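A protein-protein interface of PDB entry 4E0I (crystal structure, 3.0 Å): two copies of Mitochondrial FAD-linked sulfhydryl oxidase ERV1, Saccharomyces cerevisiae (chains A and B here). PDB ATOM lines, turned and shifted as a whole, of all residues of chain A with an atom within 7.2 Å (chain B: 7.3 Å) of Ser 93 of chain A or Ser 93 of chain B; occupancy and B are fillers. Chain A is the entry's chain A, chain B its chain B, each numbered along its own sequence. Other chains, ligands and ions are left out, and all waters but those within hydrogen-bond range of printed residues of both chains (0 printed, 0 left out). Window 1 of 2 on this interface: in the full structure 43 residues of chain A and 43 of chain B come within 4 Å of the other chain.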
ATOM      1  N   PRO A  85      -0.969  21.417  23.406  1.00  0.00           N
ATOM      2  CA  PRO A  85      -2.224  20.953  24.008  1.00  0.00           C
ATOM      3  C   PRO A  85      -2.164  19.507  24.498  1.00  0.00           C
ATOM      4  O   PRO A  85      -1.522  18.662  23.870  1.00  0.00           O
ATOM      5  CB  PRO A  85      -3.231  21.076  22.859  1.00  0.00           C
ATOM      6  CG  PRO A  85      -2.406  21.035  21.618  1.00  0.00           C
ATOM      7  CD  PRO A  85      -1.144  21.753  21.981  1.00  0.00           C
ATOM      8  N   VAL A  87      -4.204  15.841  25.885  1.00  0.00           N
ATOM      9  CA  VAL A  87      -5.296  14.980  25.412  1.00  0.00           C
ATOM     10  C   VAL A  87      -6.665  15.658  25.496  1.00  0.00           C
ATOM     11  O   VAL A  87      -7.469  15.572  24.565  1.00  0.00           O
ATOM     12  CB  VAL A  87      -5.347  13.632  26.176  1.00  0.00           C
ATOM     13  CG1 VAL A  87      -4.170  12.750  25.794  1.00  0.00           C
ATOM     14  CG2 VAL A  87      -5.384  13.847  27.686  1.00  0.00           C
ATOM     15  N   GLU A  88      -6.903  16.340  26.616  1.00  0.00           N
ATOM     16  CA  GLU A  88      -8.175  16.999  26.901  1.00  0.00           C
ATOM     17  C   GLU A  88      -8.397  18.221  26.013  1.00  0.00           C
ATOM     18  O   GLU A  88      -9.499  18.421  25.496  1.00  0.00           O
ATOM     19  CB  GLU A  88      -8.252  17.400  28.380  1.00  0.00           C
ATOM     20  CG  GLU A  88      -8.148  16.239  29.365  1.00  0.00           C
ATOM     21  CD  GLU A  88      -8.105  16.688  30.819  1.00  0.00           C
ATOM     22  OE1 GLU A  88      -8.691  17.743  31.149  1.00  0.00           O
ATOM     23  OE2 GLU A  88      -7.486  15.978  31.640  1.00  0.00           O
ATOM     24  N   GLN A  89      -7.353  19.031  25.842  1.00  0.00           N
ATOM     25  CA  GLN A  89      -7.440  20.248  25.033  1.00  0.00           C
ATOM     26  C   GLN A  89      -7.574  19.935  23.544  1.00  0.00           C
ATOM     27  O   GLN A  89      -8.422  20.514  22.862  1.00  0.00           O
ATOM     28  CB  GLN A  89      -6.249  21.181  25.300  1.00  0.00           C
ATOM     29  CG  GLN A  89      -6.275  22.499  24.530  1.00  0.00           C
ATOM     30  CD  GLN A  89      -7.593  23.248  24.648  1.00  0.00           C
ATOM     31  OE1 GLN A  89      -8.130  23.427  25.744  1.00  0.00           O
ATOM     32  NE2 GLN A  89      -8.117  23.699  23.514  1.00  0.00           N
ATOM     33  N   LEU A  90      -6.740  19.020  23.052  1.00  0.00           N
ATOM     34  CA  LEU A  90      -6.825  18.540  21.676  1.00  0.00           C
ATOM     35  C   LEU A  90      -8.178  17.884  21.411  1.00  0.00           C
ATOM     36  O   LEU A  90      -8.816  18.152  20.391  1.00  0.00           O
ATOM     37  CB  LEU A  90      -5.689  17.553  21.379  1.00  0.00           C
ATOM     38  CG  LEU A  90      -5.724  16.743  20.078  1.00  0.00           C
ATOM     39  CD1 LEU A  90      -5.509  17.629  18.857  1.00  0.00           C
ATOM     40  CD2 LEU A  90      -4.677  15.642  20.129  1.00  0.00           C
ATOM     41  N   GLY A  91      -8.603  17.032  22.343  1.00  0.00           N
ATOM     42  CA  GLY A  91      -9.874  16.325  22.245  1.00  0.00           C
ATOM     43  C   GLY A  91     -11.062  17.233  21.997  1.00  0.00           C
ATOM     44  O   GLY A  91     -11.779  17.061  21.010  1.00  0.00           O
ATOM     45  N   ARG A  92     -11.263  18.206  22.885  1.00  0.00           N
ATOM     46  CA  ARG A  92     -12.395  19.132  22.770  1.00  0.00           C
ATOM     47  C   ARG A  92     -12.248  20.111  21.603  1.00  0.00           C
ATOM     48  O   ARG A  92     -13.243  20.636  21.104  1.00  0.00           O
ATOM     49  CB  ARG A  92     -12.654  19.873  24.091  1.00  0.00           C
ATOM     50  CG  ARG A  92     -11.666  20.979  24.434  1.00  0.00           C
ATOM     51  CD  ARG A  92     -12.083  21.720  25.696  1.00  0.00           C
ATOM     52  NE  ARG A  92     -11.922  20.897  26.895  1.00  0.00           N
ATOM     53  CZ  ARG A  92     -10.811  20.836  27.626  1.00  0.00           C
ATOM     54  NH1 ARG A  92      -9.745  21.556  27.296  1.00  0.00           N
ATOM     55  NH2 ARG A  92     -10.766  20.054  28.695  1.00  0.00           N
ATOM     56  N   SER A  93     -11.008  20.347  21.177  1.00  0.00           N
ATOM     57  CA  SER A  93     -10.729  21.186  20.015  1.00  0.00           C
ATOM     58  C   SER A  93     -11.010  20.442  18.715  1.00  0.00           C
ATOM     59  O   SER A  93     -11.338  21.053  17.696  1.00  0.00           O
ATOM     60  CB  SER A  93      -9.282  21.663  20.035  1.00  0.00           C
ATOM     61  OG  SER A  93      -9.036  22.502  21.150  1.00  0.00           O
ATOM     62  N   SER A  94     -10.869  19.120  18.759  1.00  0.00           N
ATOM     63  CA  SER A  94     -11.175  18.271  17.615  1.00  0.00           C
ATOM     64  C   SER A  94     -12.682  18.075  17.473  1.00  0.00           C
ATOM     65  O   SER A  94     -13.195  17.989  16.357  1.00  0.00           O
ATOM     66  CB  SER A  94     -10.471  16.920  17.742  1.00  0.00           C
ATOM     67  OG  SER A  94      -9.069  17.081  17.865  1.00  0.00           O
ATOM     68  N   TRP A  95     -13.382  18.012  18.607  1.00  0.00           N
ATOM     69  CA  TRP A  95     -14.833  17.821  18.619  1.00  0.00           C
ATOM     70  C   TRP A  95     -15.588  19.003  18.084  1.00  0.00           C
ATOM     71  O   TRP A  95     -16.538  18.835  17.318  1.00  0.00           O
ATOM     72  CB  TRP A  95     -15.336  17.470  20.015  1.00  0.00           C
ATOM     73  CG  TRP A  95     -15.073  16.039  20.420  1.00  0.00           C
ATOM     74  CD1 TRP A  95     -14.370  15.589  21.533  1.00  0.00           C
ATOM     75  CD2 TRP A  95     -15.500  14.814  19.722  1.00  0.00           C
ATOM     76  NE1 TRP A  95     -14.337  14.219  21.575  1.00  0.00           N
ATOM     77  CE2 TRP A  95     -14.995  13.691  20.522  1.00  0.00           C
ATOM     78  CE3 TRP A  95     -16.225  14.545  18.565  1.00  0.00           C
ATOM     79  CZ2 TRP A  95     -15.212  12.370  20.156  1.00  0.00           C
ATOM     80  CZ3 TRP A  95     -16.439  13.208  18.207  1.00  0.00           C
ATOM     81  CH2 TRP A  95     -15.942  12.149  18.984  1.00  0.00           C
ATOM     82  N   THR A  96     -15.175  20.208  18.476  1.00  0.00           N
ATOM     83  CA  THR A  96     -15.828  21.430  17.999  1.00  0.00           C
ATOM     84  C   THR A  96     -15.757  21.566  16.478  1.00  0.00           C
ATOM     85  O   THR A  96     -16.717  22.021  15.856  1.00  0.00           O
ATOM     86  CB  THR A  96     -15.326  22.711  18.710  1.00  0.00           C
ATOM     87  OG1 THR A  96     -15.773  23.871  17.994  1.00  0.00           O
ATOM     88  CG2 THR A  96     -13.822  22.742  18.793  1.00  0.00           C
ATOM     89  N   LEU A  97     -14.632  21.160  15.889  1.00  0.00           N
ATOM     90  CA  LEU A  97     -14.500  21.122  14.435  1.00  0.00           C
ATOM     91  C   LEU A  97     -15.404  20.050  13.826  1.00  0.00           C
ATOM     92  O   LEU A  97     -16.191  20.345  12.924  1.00  0.00           O
ATOM     93  CB  LEU A  97     -13.039  20.906  14.011  1.00  0.00           C
ATOM     94  CG  LEU A  97     -12.744  20.703  12.517  1.00  0.00           C
ATOM     95  CD1 LEU A  97     -13.167  21.904  11.679  1.00  0.00           C
ATOM     96  CD2 LEU A  97     -11.272  20.404  12.290  1.00  0.00           C
ATOM     97  N   LEU A  98     -15.296  18.821  14.333  1.00  0.00           N
ATOM     98  CA  LEU A  98     -16.046  17.673  13.808  1.00  0.00           C
ATOM     99  C   LEU A  98     -17.564  17.875  13.797  1.00  0.00           C
ATOM    100  O   LEU A  98     -18.235  17.485  12.839  1.00  0.00           O
ATOM    101  CB  LEU A  98     -15.688  16.393  14.573  1.00  0.00           C
ATOM    102  CG  LEU A  98     -14.349  15.719  14.253  1.00  0.00           C
ATOM    103  CD1 LEU A  98     -13.948  14.771  15.374  1.00  0.00           C
ATOM    104  CD2 LEU A  98     -14.387  14.986  12.918  1.00  0.00           C
ATOM    105  N   TYR A 128      -5.017  10.979  13.686  1.00  0.00           N
ATOM    106  CA  TYR A 128      -5.337  11.614  14.963  1.00  0.00           C
ATOM    107  C   TYR A 128      -4.171  11.424  15.934  1.00  0.00           C
ATOM    108  O   TYR A 128      -3.769  10.289  16.200  1.00  0.00           O
ATOM    109  CB  TYR A 128      -6.643  11.081  15.560  1.00  0.00           C
ATOM    110  CG  TYR A 128      -7.115  11.873  16.762  1.00  0.00           C
ATOM    111  CD1 TYR A 128      -7.653  13.151  16.611  1.00  0.00           C
ATOM    112  CD2 TYR A 128      -7.015  11.350  18.051  1.00  0.00           C
ATOM    113  CE1 TYR A 128      -8.079  13.885  17.707  1.00  0.00           C
ATOM    114  CE2 TYR A 128      -7.440  12.075  19.154  1.00  0.00           C
ATOM    115  CZ  TYR A 128      -7.972  13.342  18.976  1.00  0.00           C
ATOM    116  OH  TYR A 128      -8.396  14.067  20.067  1.00  0.00           O
ATOM    117  N   PRO B  85     -19.835  27.661  17.827  1.00  0.00           N
ATOM    118  CA  PRO B  85     -18.605  28.453  17.738  1.00  0.00           C
ATOM    119  C   PRO B  85     -18.676  29.577  16.704  1.00  0.00           C
ATOM    120  O   PRO B  85     -19.278  29.406  15.641  1.00  0.00           O
ATOM    121  CB  PRO B  85     -17.548  27.423  17.311  1.00  0.00           C
ATOM    122  CG  PRO B  85     -18.143  26.092  17.620  1.00  0.00           C
ATOM    123  CD  PRO B  85     -19.614  26.265  17.413  1.00  0.00           C
ATOM    124  N   VAL B  87     -16.088  32.581  14.587  1.00  0.00           N
ATOM    125  CA  VAL B  87     -14.849  32.431  13.807  1.00  0.00           C
ATOM    126  C   VAL B  87     -13.680  32.068  14.712  1.00  0.00           C
ATOM    127  O   VAL B  87     -12.907  31.159  14.408  1.00  0.00           O
ATOM    128  CB  VAL B  87     -14.435  33.706  13.039  1.00  0.00           C
ATOM    129  CG1 VAL B  87     -13.995  33.351  11.626  1.00  0.00           C
ATOM    130  CG2 VAL B  87     -15.552  34.725  13.002  1.00  0.00           C
ATOM    131  N   GLU B  88     -13.568  32.793  15.822  1.00  0.00           N
ATOM    132  CA  GLU B  88     -12.430  32.683  16.729  1.00  0.00           C
ATOM    133  C   GLU B  88     -12.371  31.352  17.478  1.00  0.00           C
ATOM    134  O   GLU B  88     -11.296  30.760  17.599  1.00  0.00           O
ATOM    135  CB  GLU B  88     -12.410  33.859  17.710  1.00  0.00           C
ATOM    136  CG  GLU B  88     -11.914  35.164  17.105  1.00  0.00           C
ATOM    137  CD  GLU B  88     -12.029  36.346  18.053  1.00  0.00           C
ATOM    138  OE1 GLU B  88     -11.853  36.164  19.279  1.00  0.00           O
ATOM    139  OE2 GLU B  88     -12.289  37.468  17.570  1.00  0.00           O
ATOM    140  N   GLN B  89     -13.517  30.886  17.974  1.00  0.00           N
ATOM    141  CA  GLN B  89     -13.578  29.627  18.721  1.00  0.00           C
ATOM    142  C   GLN B  89     -13.310  28.420  17.824  1.00  0.00           C
ATOM    143  O   GLN B  89     -12.614  27.487  18.224  1.00  0.00           O
ATOM    144  CB  GLN B  89     -14.922  29.477  19.446  1.00  0.00           C
ATOM    145  CG  GLN B  89     -14.946  28.380  20.504  1.00  0.00           C
ATOM    146  CD  GLN B  89     -13.956  28.622  21.631  1.00  0.00           C
ATOM    147  OE1 GLN B  89     -14.101  29.566  22.410  1.00  0.00           O
ATOM    148  NE2 GLN B  89     -12.946  27.765  21.725  1.00  0.00           N
ATOM    149  N   LEU B  90     -13.866  28.453  16.615  1.00  0.00           N
ATOM    150  CA  LEU B  90     -13.647  27.414  15.614  1.00  0.00           C
ATOM    151  C   LEU B  90     -12.230  27.484  15.051  1.00  0.00           C
ATOM    152  O   LEU B  90     -11.599  26.452  14.811  1.00  0.00           O
ATOM    153  CB  LEU B  90     -14.675  27.551  14.486  1.00  0.00           C
ATOM    154  CG  LEU B  90     -14.556  26.698  13.220  1.00  0.00           C
ATOM    155  CD1 LEU B  90     -14.988  25.261  13.474  1.00  0.00           C
ATOM    156  CD2 LEU B  90     -15.384  27.324  12.110  1.00  0.00           C
ATOM    157  N   GLY B  91     -11.743  28.707  14.850  1.00  0.00           N
ATOM    158  CA  GLY B  91     -10.421  28.953  14.279  1.00  0.00           C
ATOM    159  C   GLY B  91      -9.294  28.352  15.093  1.00  0.00           C
ATOM    160  O   GLY B  91      -8.552  27.501  14.596  1.00  0.00           O
ATOM    161  N   ARG B  92      -9.175  28.785  16.347  1.00  0.00           N
ATOM    162  CA  ARG B  92      -8.129  28.289  17.249  1.00  0.00           C
ATOM    163  C   ARG B  92      -8.242  26.785  17.510  1.00  0.00           C
ATOM    164  O   ARG B  92      -7.246  26.130  17.813  1.00  0.00           O
ATOM    165  CB  ARG B  92      -8.110  29.080  18.567  1.00  0.00           C
ATOM    166  CG  ARG B  92      -9.307  28.861  19.483  1.00  0.00           C
ATOM    167  CD  ARG B  92      -9.197  29.691  20.753  1.00  0.00           C
ATOM    168  NE  ARG B  92      -9.499  31.103  20.521  1.00  0.00           N
ATOM    169  CZ  ARG B  92     -10.676  31.676  20.770  1.00  0.00           C
ATOM    170  NH1 ARG B  92     -11.680  30.968  21.269  1.00  0.00           N
ATOM    171  NH2 ARG B  92     -10.844  32.968  20.526  1.00  0.00           N
ATOM    172  N   SER B  93      -9.457  26.253  17.381  1.00  0.00           N
ATOM    173  CA  SER B  93      -9.711  24.822  17.529  1.00  0.00           C
ATOM    174  C   SER B  93      -9.272  24.035  16.299  1.00  0.00           C
ATOM    175  O   SER B  93      -8.829  22.890  16.409  1.00  0.00           O
ATOM    176  CB  SER B  93     -11.193  24.572  17.794  1.00  0.00           C
ATOM    177  OG  SER B  93     -11.593  25.156  19.020  1.00  0.00           O
ATOM    178  N   SER B  94      -9.412  24.651  15.128  1.00  0.00           N
ATOM    179  CA  SER B  94      -8.982  24.035  13.880  1.00  0.00           C
ATOM    180  C   SER B  94      -7.464  24.096  13.746  1.00  0.00           C
ATOM    181  O   SER B  94      -6.841  23.138  13.286  1.00  0.00           O
ATOM    182  CB  SER B  94      -9.659  24.706  12.683  1.00  0.00           C
ATOM    183  OG  SER B  94     -11.069  24.602  12.777  1.00  0.00           O
ATOM    184  N   TRP B  95      -6.878  25.219  14.160  1.00  0.00           N
ATOM    185  CA  TRP B  95      -5.426  25.392  14.144  1.00  0.00           C
ATOM    186  C   TRP B  95      -4.724  24.457  15.082  1.00  0.00           C
ATOM    187  O   TRP B  95      -3.683  23.898  14.735  1.00  0.00           O
ATOM    188  CB  TRP B  95      -5.040  26.833  14.455  1.00  0.00           C
ATOM    189  CG  TRP B  95      -5.319  27.792  13.325  1.00  0.00           C
ATOM    190  CD1 TRP B  95      -6.110  28.936  13.359  1.00  0.00           C
ATOM    191  CD2 TRP B  95      -4.810  27.723  11.945  1.00  0.00           C
ATOM    192  NE1 TRP B  95      -6.125  29.560  12.137  1.00  0.00           N
ATOM    193  CE2 TRP B  95      -5.365  28.889  11.247  1.00  0.00           C
ATOM    194  CE3 TRP B  95      -3.979  26.852  11.249  1.00  0.00           C
ATOM    195  CZ2 TRP B  95      -5.093  29.143   9.910  1.00  0.00           C
ATOM    196  CZ3 TRP B  95      -3.712  27.119   9.900  1.00  0.00           C
ATOM    197  CH2 TRP B  95      -4.258  28.237   9.249  1.00  0.00           C
ATOM    198  N   THR B  96      -5.287  24.268  16.275  1.00  0.00           N
ATOM    199  CA  THR B  96      -4.694  23.359  17.257  1.00  0.00           C
ATOM    200  C   THR B  96      -4.705  21.902  16.790  1.00  0.00           C
ATOM    201  O   THR B  96      -3.805  21.139  17.133  1.00  0.00           O
ATOM    202  CB  THR B  96      -5.301  23.506  18.676  1.00  0.00           C
ATOM    203  OG1 THR B  96      -4.588  22.671  19.596  1.00  0.00           O
ATOM    204  CG2 THR B  96      -6.753  23.119  18.701  1.00  0.00           C
ATOM    205  N   LEU B  97      -5.714  21.527  16.003  1.00  0.00           N
ATOM    206  CA  LEU B  97      -5.753  20.199  15.400  1.00  0.00           C
ATOM    207  C   LEU B  97      -4.754  20.094  14.252  1.00  0.00           C
ATOM    208  O   LEU B  97      -3.930  19.178  14.229  1.00  0.00           O
ATOM    209  CB  LEU B  97      -7.161  19.837  14.915  1.00  0.00           C
ATOM    210  CG  LEU B  97      -7.282  18.494  14.182  1.00  0.00           C
ATOM    211  CD1 LEU B  97      -7.082  17.314  15.124  1.00  0.00           C
ATOM    212  CD2 LEU B  97      -8.622  18.384  13.475  1.00  0.00           C
ATOM    213  N   LEU B  98      -4.832  21.035  13.311  1.00  0.00           N
ATOM    214  CA  LEU B  98      -3.951  21.055  12.141  1.00  0.00           C
ATOM    215  C   LEU B  98      -2.475  21.016  12.532  1.00  0.00           C
ATOM    216  O   LEU B  98      -1.694  20.263  11.948  1.00  0.00           O
ATOM    217  CB  LEU B  98      -4.236  22.276  11.255  1.00  0.00           C
ATOM    218  CG  LEU B  98      -5.577  22.368  10.514  1.00  0.00           C
ATOM    219  CD1 LEU B  98      -5.799  23.779   9.986  1.00  0.00           C
ATOM    220  CD2 LEU B  98      -5.687  21.349   9.388  1.00  0.00           C
ATOM    221  N   TYR B 128     -14.633  23.020   5.382  1.00  0.00           N
ATOM    222  CA  TYR B 128     -14.479  23.939   6.518  1.00  0.00           C
ATOM    223  C   TYR B 128     -15.750  24.775   6.705  1.00  0.00           C
ATOM    224  O   TYR B 128     -16.285  25.303   5.726  1.00  0.00           O
ATOM    225  CB  TYR B 128     -13.245  24.838   6.352  1.00  0.00           C
ATOM    226  CG  TYR B 128     -12.933  25.680   7.577  1.00  0.00           C
ATOM    227  CD1 TYR B 128     -12.313  25.117   8.695  1.00  0.00           C
ATOM    228  CD2 TYR B 128     -13.262  27.034   7.621  1.00  0.00           C
ATOM    229  CE1 TYR B 128     -12.034  25.879   9.820  1.00  0.00           C
ATOM    230  CE2 TYR B 128     -12.984  27.804   8.742  1.00  0.00           C
ATOM    231  CZ  TYR B 128     -12.371  27.222   9.837  1.00  0.00           C
ATOM    232  OH  TYR B 128     -12.092  27.982  10.950  1.00  0.00           O
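The backbone carbonyl oxygen (O) of Ser 93 of chain A lies close to the backbone carbonyl oxygen (O) of Ser 93 of chain B (3.4 Å).
OG of Ser 93 of chain B sits at hydrogen-bond distance from O of Gln 89 of chain B, at 2.7 Å.
OG of Ser 94 of chain A is in hydrogen-bond range of O of Leu 90 of chain A, 2.8 Å away.
The backbone carbonyl oxygen (O) of Leu 90 of chain B sits at hydrogen-bond distance from the side-chain hydroxyl (OG) of Ser 94 of chain B, 2.8 Å away.
OG of Ser 93 of chain A is in hydrogen-bond range of O of Gln 89 of chain A (2.7 Å).
Thr 96 of chain B touches Pro 85 of chain A.
Ser 93 of chain A touches Thr 96 of chain B.
CD1 of Leu 97 of chain B touches OG of Ser 94 of chain A (3.4 Å).
CG of Pro 85 of chain B touches OG1 of Thr 96 of chain A (3.3 Å).
Ser 93 of chain B touches Thr 96 of chain A (OG to CG2, 3.3 Å).
Leu 97 of chain A touches Ser 94 of chain B.
Leu 97 of chain A touches Leu 97 of chain B (CD2 to CD2, 3.5 Å).
Ser 93 of chain A touches just these residues of chain B: Ser 93 (3.4 Å) and Thr 96 (3.2 Å).
Of the printed residues of chain B, Leu 97 of chain A touches Ser 94 and Leu 97.
Printed residues of chain B within 4 Å of Ser 94 of chain A: Leu 97 (3.4 Å).
Of the printed residues of chain A, Thr 96 of chain B touches Pro 85 (3.4 Å) and Ser 93 (3.2 Å).
Printed residues of chain B within 4 Å of Pro 85 of chain A: Thr 96.
Arg 92 of chain B touches none of the printed residues of chain A.
Gly 91 of chain A touches none of the printed residues of chain B.
The nearest printed residue of chain A that does not touch Thr 96 of chain B is Leu 90 of chain A (4.3 Å).
Of the 14 printed residues of chain B, 5 touch a printed residue of chain A.
Hydrophobic or aromatic side chains of chain B that line the printed part of chain A: Pro 85 and Leu 97.
Of the 14 printed residues of chain A, 5 touch a printed residue of chain B.
Hydrophobic or aromatic side chains of chain A within 4 Å of the printed part of chain B: Pro 85 and Leu 97.
Among the printed residues, no Asp or Glu carboxylate lies within 4 Å of a Lys or Arg side-chain nitrogen of the other chain.
Pro 85 of chain A touches Thr 96 of chain B, and with the chains exchanged Thr 96 of chain A touches Pro 85 of chain B.
Ser 93 of chain B touches its own counterpart, Ser 93 of chain A.
Ser 93 of chain A touches Thr 96 of chain B, and with the chains exchanged Thr 96 of chain A touches Ser 93 of chain B.
Ser 94 of chain A touches Leu 97 of chain B, and with the chains exchanged Leu 97 of chain A touches Ser 94 of chain B.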
